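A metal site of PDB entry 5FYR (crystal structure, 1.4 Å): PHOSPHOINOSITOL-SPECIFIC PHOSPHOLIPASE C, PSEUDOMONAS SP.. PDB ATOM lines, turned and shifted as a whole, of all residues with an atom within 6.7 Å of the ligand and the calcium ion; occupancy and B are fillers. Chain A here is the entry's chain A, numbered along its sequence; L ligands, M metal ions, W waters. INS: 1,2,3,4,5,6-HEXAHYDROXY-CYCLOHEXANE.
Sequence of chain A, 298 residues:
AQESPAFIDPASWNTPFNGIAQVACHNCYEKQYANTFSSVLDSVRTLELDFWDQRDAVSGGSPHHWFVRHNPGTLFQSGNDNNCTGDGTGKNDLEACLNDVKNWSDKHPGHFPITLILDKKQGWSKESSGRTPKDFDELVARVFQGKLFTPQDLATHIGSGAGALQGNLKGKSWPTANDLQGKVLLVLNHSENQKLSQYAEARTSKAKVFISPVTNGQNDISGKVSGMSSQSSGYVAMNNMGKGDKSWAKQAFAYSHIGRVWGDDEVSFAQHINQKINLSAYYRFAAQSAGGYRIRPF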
ATOM      1  N   CYS A  25       4.648 -24.755  24.447  1.00  0.00           N
ATOM      2  CA  CYS A  25       3.644 -24.384  25.410  1.00  0.00           C
ATOM      3  C   CYS A  25       2.767 -23.233  24.931  1.00  0.00           C
ATOM      4  O   CYS A  25       3.161 -22.447  24.024  1.00  0.00           O
ATOM      5  CB  CYS A  25       4.276 -24.024  26.747  1.00  0.00           C
ATOM      6  SG  CYS A  25       4.626 -22.291  26.955  1.00  0.00           S
ATOM      7  N   HIS A  26       1.578 -23.125  25.520  1.00  0.00           N
ATOM      8  CA  HIS A  26       0.778 -21.945  25.365  1.00  0.00           C
ATOM      9  C   HIS A  26       0.559 -21.339  26.770  1.00  0.00           C
ATOM     10  O   HIS A  26      -0.075 -21.946  27.651  1.00  0.00           O
ATOM     11  CB  HIS A  26      -0.566 -22.314  24.734  1.00  0.00           C
ATOM     12  CG  HIS A  26      -1.465 -21.145  24.456  1.00  0.00           C
ATOM     13  ND1 HIS A  26      -2.675 -21.297  23.830  1.00  0.00           N
ATOM     14  CD2 HIS A  26      -1.306 -19.798  24.634  1.00  0.00           C
ATOM     15  CE1 HIS A  26      -3.277 -20.118  23.713  1.00  0.00           C
ATOM     16  NE2 HIS A  26      -2.463 -19.195  24.189  1.00  0.00           N
ATOM     17  N   ASN A  27       1.133 -20.150  26.981  1.00  0.00           N
ATOM     18  CA  ASN A  27       0.959 -19.420  28.224  1.00  0.00           C
ATOM     19  C   ASN A  27       1.463 -20.179  29.430  1.00  0.00           C
ATOM     20  O   ASN A  27       0.929 -20.069  30.533  1.00  0.00           O
ATOM     21  CB  ASN A  27      -0.453 -18.957  28.438  1.00  0.00           C
ATOM     22  CG  ASN A  27      -0.885 -17.798  27.571  1.00  0.00           C
ATOM     23  OD1 ASN A  27      -0.183 -17.297  26.706  1.00  0.00           O
ATOM     24  ND2 ASN A  27      -2.055 -17.336  27.852  1.00  0.00           N
ATOM     25  N   TYR A  29       3.768 -19.755  31.528  1.00  0.00           N
ATOM     26  CA  TYR A  29       4.087 -18.925  32.685  1.00  0.00           C
ATOM     27  C   TYR A  29       2.952 -18.890  33.704  1.00  0.00           C
ATOM     28  O   TYR A  29       3.164 -18.446  34.849  1.00  0.00           O
ATOM     29  CB  TYR A  29       4.379 -17.463  32.258  1.00  0.00           C
ATOM     30  CG  TYR A  29       3.193 -16.749  31.715  1.00  0.00           C
ATOM     31  CD1 TYR A  29       2.298 -16.111  32.586  1.00  0.00           C
ATOM     32  CD2 TYR A  29       2.888 -16.765  30.358  1.00  0.00           C
ATOM     33  CE1 TYR A  29       1.175 -15.503  32.090  1.00  0.00           C
ATOM     34  CE2 TYR A  29       1.742 -16.194  29.861  1.00  0.00           C
ATOM     35  CZ  TYR A  29       0.871 -15.560  30.731  1.00  0.00           C
ATOM     36  OH  TYR A  29      -0.299 -14.958  30.313  1.00  0.00           O
ATOM     37  N   GLU A  48       6.564 -19.586  26.346  1.00  0.00           N
ATOM     38  CA  GLU A  48       5.858 -18.346  26.128  1.00  0.00           C
ATOM     39  C   GLU A  48       5.775 -17.490  27.397  1.00  0.00           C
ATOM     40  O   GLU A  48       5.518 -18.017  28.468  1.00  0.00           O
ATOM     41  CB  GLU A  48       4.447 -18.654  25.578  1.00  0.00           C
ATOM     42  CG  GLU A  48       3.627 -17.398  25.231  1.00  0.00           C
ATOM     43  CD  GLU A  48       2.282 -17.708  24.568  1.00  0.00           C
ATOM     44  OE1 GLU A  48       1.860 -18.892  24.516  1.00  0.00           O
ATOM     45  OE2 GLU A  48       1.606 -16.723  24.120  1.00  0.00           O
ATOM     46  N   LEU A  49       5.917 -16.181  27.225  1.00  0.00           N
ATOM     47  CA  LEU A  49       5.748 -15.186  28.262  1.00  0.00           C
ATOM     48  C   LEU A  49       4.883 -14.077  27.710  1.00  0.00           C
ATOM     49  O   LEU A  49       5.199 -13.505  26.657  1.00  0.00           O
ATOM     50  CB  LEU A  49       7.108 -14.621  28.678  1.00  0.00           C
ATOM     51  CG  LEU A  49       7.975 -15.570  29.448  1.00  0.00           C
ATOM     52  CD1 LEU A  49       9.435 -15.152  29.451  1.00  0.00           C
ATOM     53  CD2 LEU A  49       7.485 -15.819  30.875  1.00  0.00           C
ATOM     54  N   ASP A  50       3.847 -13.698  28.448  1.00  0.00           N
ATOM     55  CA  ASP A  50       3.043 -12.508  28.127  1.00  0.00           C
ATOM     56  C   ASP A  50       3.544 -11.356  28.986  1.00  0.00           C
ATOM     57  O   ASP A  50       3.518 -11.458  30.195  1.00  0.00           O
ATOM     58  CB  ASP A  50       1.560 -12.788  28.428  1.00  0.00           C
ATOM     59  CG  ASP A  50       0.942 -13.839  27.496  1.00  0.00           C
ATOM     60  OD1 ASP A  50       1.639 -14.380  26.626  1.00  0.00           O
ATOM     61  OD2 ASP A  50      -0.209 -14.206  27.628  1.00  0.00           O
ATOM     62  N   HIS A  70      -1.289 -12.728  32.734  1.00  0.00           N
ATOM     63  CA  HIS A  70      -2.233 -12.939  31.655  1.00  0.00           C
ATOM     64  C   HIS A  70      -3.225 -11.779  31.411  1.00  0.00           C
ATOM     65  O   HIS A  70      -3.339 -11.301  30.308  1.00  0.00           O
ATOM     66  CB  HIS A  70      -3.000 -14.232  31.979  1.00  0.00           C
ATOM     67  CG  HIS A  70      -3.879 -14.667  30.866  1.00  0.00           C
ATOM     68  ND1 HIS A  70      -5.191 -15.047  31.055  1.00  0.00           N
ATOM     69  CD2 HIS A  70      -3.655 -14.721  29.543  1.00  0.00           C
ATOM     70  CE1 HIS A  70      -5.725 -15.353  29.886  1.00  0.00           C
ATOM     71  NE2 HIS A  70      -4.805 -15.185  28.965  1.00  0.00           N
ATOM     72  N   ILE A 117       8.707 -17.357  23.072  1.00  0.00           N
ATOM     73  CA  ILE A 117       7.719 -16.498  22.463  1.00  0.00           C
ATOM     74  C   ILE A 117       7.405 -15.413  23.492  1.00  0.00           C
ATOM     75  O   ILE A 117       6.870 -15.696  24.577  1.00  0.00           O
ATOM     76  CB  ILE A 117       6.435 -17.276  22.128  1.00  0.00           C
ATOM     77  CG1 ILE A 117       6.748 -18.539  21.201  1.00  0.00           C
ATOM     78  CG2 ILE A 117       5.341 -16.319  21.661  1.00  0.00           C
ATOM     79  CD1 ILE A 117       7.501 -18.307  19.972  1.00  0.00           C
ATOM     80  N   ASP A 119       5.146 -12.480  24.095  1.00  0.00           N
ATOM     81  CA  ASP A 119       3.865 -12.041  23.617  1.00  0.00           C
ATOM     82  C   ASP A 119       3.553 -10.682  24.273  1.00  0.00           C
ATOM     83  O   ASP A 119       3.211 -10.634  25.463  1.00  0.00           O
ATOM     84  CB  ASP A 119       2.847 -13.127  23.922  1.00  0.00           C
ATOM     85  CG  ASP A 119       1.465 -12.808  23.414  1.00  0.00           C
ATOM     86  OD1 ASP A 119       1.344 -12.023  22.465  1.00  0.00           O
ATOM     87  OD2 ASP A 119       0.471 -13.400  23.940  1.00  0.00           O
ATOM     88  N   LYS A 120       3.829  -9.604  23.545  1.00  0.00           N
ATOM     89  CA  LYS A 120       3.731  -8.255  24.068  1.00  0.00           C
ATOM     90  C   LYS A 120       2.273  -7.863  24.156  1.00  0.00           C
ATOM     91  O   LYS A 120       1.541  -8.049  23.167  1.00  0.00           O
ATOM     92  CB  LYS A 120       4.524  -7.301  23.188  1.00  0.00           C
ATOM     93  CG  LYS A 120       4.746  -5.949  23.849  1.00  0.00           C
ATOM     94  CD  LYS A 120       5.569  -5.011  22.939  1.00  0.00           C
ATOM     95  CE  LYS A 120       6.199  -3.833  23.705  1.00  0.00           C
ATOM     96  NZ  LYS A 120       5.389  -3.295  24.787  1.00  0.00           N
ATOM     97  N   LYS A 121       1.847  -7.272  25.288  1.00  0.00           N
ATOM     98  CA  LYS A 121       0.444  -6.982  25.508  1.00  0.00           C
ATOM     99  C   LYS A 121       0.059  -5.501  25.462  1.00  0.00           C
ATOM    100  O   LYS A 121      -1.131  -5.181  25.363  1.00  0.00           O
ATOM    101  CB  LYS A 121       0.002  -7.586  26.843  1.00  0.00           C
ATOM    102  CG  LYS A 121       0.089  -9.108  26.870  1.00  0.00           C
ATOM    103  CD  LYS A 121      -0.960  -9.737  25.933  1.00  0.00           C
ATOM    104  CE  LYS A 121      -0.937 -11.244  25.942  1.00  0.00           C
ATOM    105  NZ  LYS A 121      -1.919 -11.829  24.962  1.00  0.00           N
ATOM    106  N   ASN A 189       5.716 -11.415  19.561  1.00  0.00           N
ATOM    107  CA  ASN A 189       4.351 -11.440  19.068  1.00  0.00           C
ATOM    108  C   ASN A 189       3.580 -10.245  19.679  1.00  0.00           C
ATOM    109  O   ASN A 189       3.976  -9.682  20.706  1.00  0.00           O
ATOM    110  CB  ASN A 189       3.535 -12.688  19.470  1.00  0.00           C
ATOM    111  CG  ASN A 189       4.023 -14.000  18.899  1.00  0.00           C
ATOM    112  OD1 ASN A 189       4.862 -14.080  17.950  1.00  0.00           O
ATOM    113  ND2 ASN A 189       3.556 -15.052  19.462  1.00  0.00           N
ATOM    114  N   HIS A 190       2.507  -9.851  19.031  1.00  0.00           N
ATOM    115  CA  HIS A 190       1.539  -8.853  19.519  1.00  0.00           C
ATOM    116  C   HIS A 190       0.272  -9.104  18.685  1.00  0.00           C
ATOM    117  O   HIS A 190       0.363  -9.548  17.549  1.00  0.00           O
ATOM    118  CB  HIS A 190       2.101  -7.436  19.315  1.00  0.00           C
ATOM    119  CG  HIS A 190       1.377  -6.384  20.074  1.00  0.00           C
ATOM    120  ND1 HIS A 190       0.178  -5.872  19.648  1.00  0.00           N
ATOM    121  CD2 HIS A 190       1.663  -5.707  21.220  1.00  0.00           C
ATOM    122  CE1 HIS A 190      -0.273  -4.976  20.495  1.00  0.00           C
ATOM    123  NE2 HIS A 190       0.611  -4.838  21.454  1.00  0.00           N
ATOM    124  N   SER A 191      -0.879  -8.695  19.194  1.00  0.00           N
ATOM    125  CA  SER A 191      -2.119  -8.781  18.425  1.00  0.00           C
ATOM    126  C   SER A 191      -2.130  -7.830  17.248  1.00  0.00           C
ATOM    127  O   SER A 191      -2.782  -8.079  16.271  1.00  0.00           O
ATOM    128  CB  SER A 191      -3.322  -8.603  19.363  1.00  0.00           C
ATOM    129  OG  SER A 191      -3.402  -7.287  19.772  1.00  0.00           O
ATOM    130  N   VAL A 214       1.162 -11.717  12.965  1.00  0.00           N
ATOM    131  CA  VAL A 214      -0.124 -12.355  12.746  1.00  0.00           C
ATOM    132  C   VAL A 214      -0.239 -12.572  11.247  1.00  0.00           C
ATOM    133  O   VAL A 214      -0.047 -11.631  10.462  1.00  0.00           O
ATOM    134  CB  VAL A 214      -1.283 -11.466  13.217  1.00  0.00           C
ATOM    135  CG1 VAL A 214      -2.635 -12.076  12.858  1.00  0.00           C
ATOM    136  CG2 VAL A 214      -1.194 -11.254  14.726  1.00  0.00           C
ATOM    137  N   ASN A 240       3.147 -16.242  12.803  1.00  0.00           N
ATOM    138  CA  ASN A 240       2.300 -16.677  13.934  1.00  0.00           C
ATOM    139  C   ASN A 240       0.838 -16.797  13.458  1.00  0.00           C
ATOM    140  O   ASN A 240       0.292 -15.848  12.925  1.00  0.00           O
ATOM    141  CB  ASN A 240       2.398 -15.702  15.117  1.00  0.00           C
ATOM    142  CG  ASN A 240       2.121 -16.379  16.481  1.00  0.00           C
ATOM    143  OD1 ASN A 240       2.683 -17.438  16.828  1.00  0.00           O
ATOM    144  ND2 ASN A 240       1.255 -15.761  17.254  1.00  0.00           N
ATOM    145  N   ARG A 260       4.325 -20.928  13.726  1.00  0.00           N
ATOM    146  CA  ARG A 260       3.726 -21.327  14.986  1.00  0.00           C
ATOM    147  C   ARG A 260       2.207 -21.229  14.890  1.00  0.00           C
ATOM    148  O   ARG A 260       1.669 -20.257  14.373  1.00  0.00           O
ATOM    149  CB  ARG A 260       4.223 -20.414  16.131  1.00  0.00           C
ATOM    150  CG  ARG A 260       3.644 -20.740  17.502  1.00  0.00           C
ATOM    151  CD  ARG A 260       4.433 -20.058  18.618  1.00  0.00           C
ATOM    152  NE  ARG A 260       3.859 -20.179  19.958  1.00  0.00           N
ATOM    153  CZ  ARG A 260       2.840 -19.446  20.366  1.00  0.00           C
ATOM    154  NH1 ARG A 260       2.255 -18.565  19.570  1.00  0.00           N
ATOM    155  NH2 ARG A 260       2.440 -19.551  21.621  1.00  0.00           N
ATOM    156  N   TRP A 262      -1.239 -21.530  17.400  1.00  0.00           N
ATOM    157  CA  TRP A 262      -1.767 -21.547  18.754  1.00  0.00           C
ATOM    158  C   TRP A 262      -3.284 -21.672  18.704  1.00  0.00           C
ATOM    159  O   TRP A 262      -3.905 -21.349  17.700  1.00  0.00           O
ATOM    160  CB  TRP A 262      -1.381 -20.253  19.511  1.00  0.00           C
ATOM    161  CG  TRP A 262      -1.846 -18.985  18.844  1.00  0.00           C
ATOM    162  CD1 TRP A 262      -1.174 -18.270  17.897  1.00  0.00           C
ATOM    163  CD2 TRP A 262      -3.041 -18.263  19.103  1.00  0.00           C
ATOM    164  NE1 TRP A 262      -1.884 -17.175  17.527  1.00  0.00           N
ATOM    165  CE2 TRP A 262      -3.023 -17.119  18.258  1.00  0.00           C
ATOM    166  CE3 TRP A 262      -4.119 -18.430  19.973  1.00  0.00           C
ATOM    167  CZ2 TRP A 262      -4.062 -16.183  18.213  1.00  0.00           C
ATOM    168  CZ3 TRP A 262      -5.143 -17.480  19.937  1.00  0.00           C
ATOM    169  CH2 TRP A 262      -5.101 -16.384  19.067  1.00  0.00           C
ATOM    170  N   GLY A 263      -3.842 -22.185  19.801  1.00  0.00           N
ATOM    171  CA  GLY A 263      -5.284 -22.340  19.972  1.00  0.00           C
ATOM    172  C   GLY A 263      -5.868 -23.600  19.346  1.00  0.00           C
ATOM    173  O   GLY A 263      -7.083 -23.736  19.292  1.00  0.00           O
ATOM    174  N   ALA A 281       1.483 -24.898  19.676  1.00  0.00           N
ATOM    175  CA  ALA A 281       1.344 -24.440  21.045  1.00  0.00           C
ATOM    176  C   ALA A 281       0.159 -25.077  21.734  1.00  0.00           C
ATOM    177  O   ALA A 281      -0.965 -24.974  21.237  1.00  0.00           O
ATOM    178  CB  ALA A 281       1.252 -22.906  21.071  1.00  0.00           C
ATOM    179  N   TYR A 283      -1.793 -25.733  25.708  1.00  0.00           N
ATOM    180  CA  TYR A 283      -1.880 -25.527  27.134  1.00  0.00           C
ATOM    181  C   TYR A 283      -1.360 -26.724  27.886  1.00  0.00           C
ATOM    182  O   TYR A 283      -0.513 -26.586  28.828  1.00  0.00           O
ATOM    183  CB  TYR A 283      -3.304 -25.279  27.564  1.00  0.00           C
ATOM    184  CG  TYR A 283      -3.950 -24.026  27.022  1.00  0.00           C
ATOM    185  CD1 TYR A 283      -3.488 -22.770  27.404  1.00  0.00           C
ATOM    186  CD2 TYR A 283      -5.021 -24.079  26.145  1.00  0.00           C
ATOM    187  CE1 TYR A 283      -4.075 -21.621  26.939  1.00  0.00           C
ATOM    188  CE2 TYR A 283      -5.609 -22.932  25.657  1.00  0.00           C
ATOM    189  CZ  TYR A 283      -5.166 -21.687  26.086  1.00  0.00           C
ATOM    190  OH  TYR A 283      -5.775 -20.524  25.611  1.00  0.00           O
HETATM  191  C1  INS L   1      -2.633 -15.180  21.795  1.00  0.00           C
HETATM  192  C2  INS L   1      -1.886 -16.424  22.264  1.00  0.00           C
HETATM  193  C3  INS L   1      -0.668 -16.764  21.480  1.00  0.00           C
HETATM  194  C4  INS L   1       0.120 -15.599  21.016  1.00  0.00           C
HETATM  195  C5  INS L   1      -0.589 -14.371  20.620  1.00  0.00           C
HETATM  196  C6  INS L   1      -1.781 -14.026  21.394  1.00  0.00           C
HETATM  197  O1  INS L   1      -3.465 -14.820  22.903  1.00  0.00           O
HETATM  198  O2  INS L   1      -1.479 -16.137  23.615  1.00  0.00           O
HETATM  199  O3  INS L   1       0.104 -17.798  22.091  1.00  0.00           O
HETATM  200  O4  INS L   1       1.194 -15.994  20.207  1.00  0.00           O
HETATM  201  O5  INS L   1       0.213 -13.283  20.192  1.00  0.00           O
HETATM  202  O6  INS L   1      -2.472 -12.899  20.968  1.00  0.00           O
HETATM  203 CA    CA M   1       0.103 -15.398  25.257  1.00  0.00          CA
HETATM  204  O   HOH W   1      -1.116 -10.911  22.385  1.00  0.00           O
HETATM  205  O   HOH W   2      -2.171 -12.323  18.131  1.00  0.00           O
HETATM  206  O   HOH W   3       0.319 -13.010  17.361  1.00  0.00           O
HETATM  207  O   HOH W   4      -3.714 -16.679  24.824  1.00  0.00           O
HETATM  208  O   HOH W   5      -2.231 -14.630  25.607  1.00  0.00           O
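The guanidinium group (NH1) of Arg 260 lies within hydrogen-bond range of an oxygen (O4) of the ligand (2.9 Å). A ring nitrogen (NE2) of His 26 sits close to an oxygen (O2) of the ligand (3.3 Å). The side-chain amide nitrogen of Asn 240 sits at hydrogen-bond distance from an oxygen (O4) of the ligand (3.0 Å). The side-chain amide nitrogen (ND2) of Asn 189 lies within hydrogen-bond range of an oxygen (O4) of the ligand.
NH2 of Arg 260 is in salt-bridge range of OE1 of Glu 48 (3.0 Å). ND2 of Asn 189 sits close to ND2 of Asn 240, at 3.3 Å. NH1 of Arg 260 sits at hydrogen-bond distance from OD1 of Asn 240 (3.0 Å). N of Glu 48 sits at hydrogen-bond distance from SG of Cys 25 (3.4 Å). The side-chain carboxylate (OD2) of Asp 119 sits close to the side-chain amino group (NZ) of Lys 121. The backbone NH (N) of Asp 119 is in hydrogen-bond range of the backbone carbonyl oxygen (O) of Leu 49 (2.8 Å). The side-chain carboxylate (OD2) of Asp 50 sits close to the side-chain amino group (NZ) of Lys 121 (3.96 Å). The side-chain carboxylate of Asp 50 sits close to the side-chain hydroxyl of Tyr 29 (2.8 Å).
Residues that only touch the ligand: Lys 121 and Trp 262. Hydrophobic or aromatic side chains within 4 Å of the ligand: His 26 and Trp 262. Within 4 Å of the ligand: His 26, Asn 27, Glu 48, Asp 119, Lys 121, Asn 189, Asn 240, Arg 260 and Trp 262.
Along chain A the residues within 4 Å of the calcium ion span positions 27 to 119. The nearest printed residue that does not touch the calcium ion is Lys 121 (4.1 Å).
The side-chain carboxylate (OD1) of Asp 50 is bound to the calcium ion (2.3 Å). OE2 of Glu 48 binds the calcium ion (2.3 Å). O2 of the ligand binds the calcium ion, 2.4 Å away. OD1 of Asn 27 is bound to the calcium ion (2.4 Å). OD2 of Asp 119 is bound to the calcium ion (2.4 Å). Water W5 binds the calcium ion (2.5 Å). OD2 of Asp 50 is bound to the calcium ion (2.7 Å).
Water W5 bridges the side-chain amino group (NZ) of Lys 121 and an oxygen (O1) of the ligand. Water W4 lies within hydrogen-bond range of O1 of the ligand and NE2 of His 26. Water W1 lies within hydrogen-bond range of OD1 of Asp 119, O6 of the ligand and NZ of Lys 121. Water W3 lies within hydrogen-bond range of an oxygen (O5) of the ligand (2.8 Å), the side-chain amide nitrogen (ND2) of Asn 240 (2.9 Å) and the backbone carbonyl oxygen (O) of His 190 (3.5 Å).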
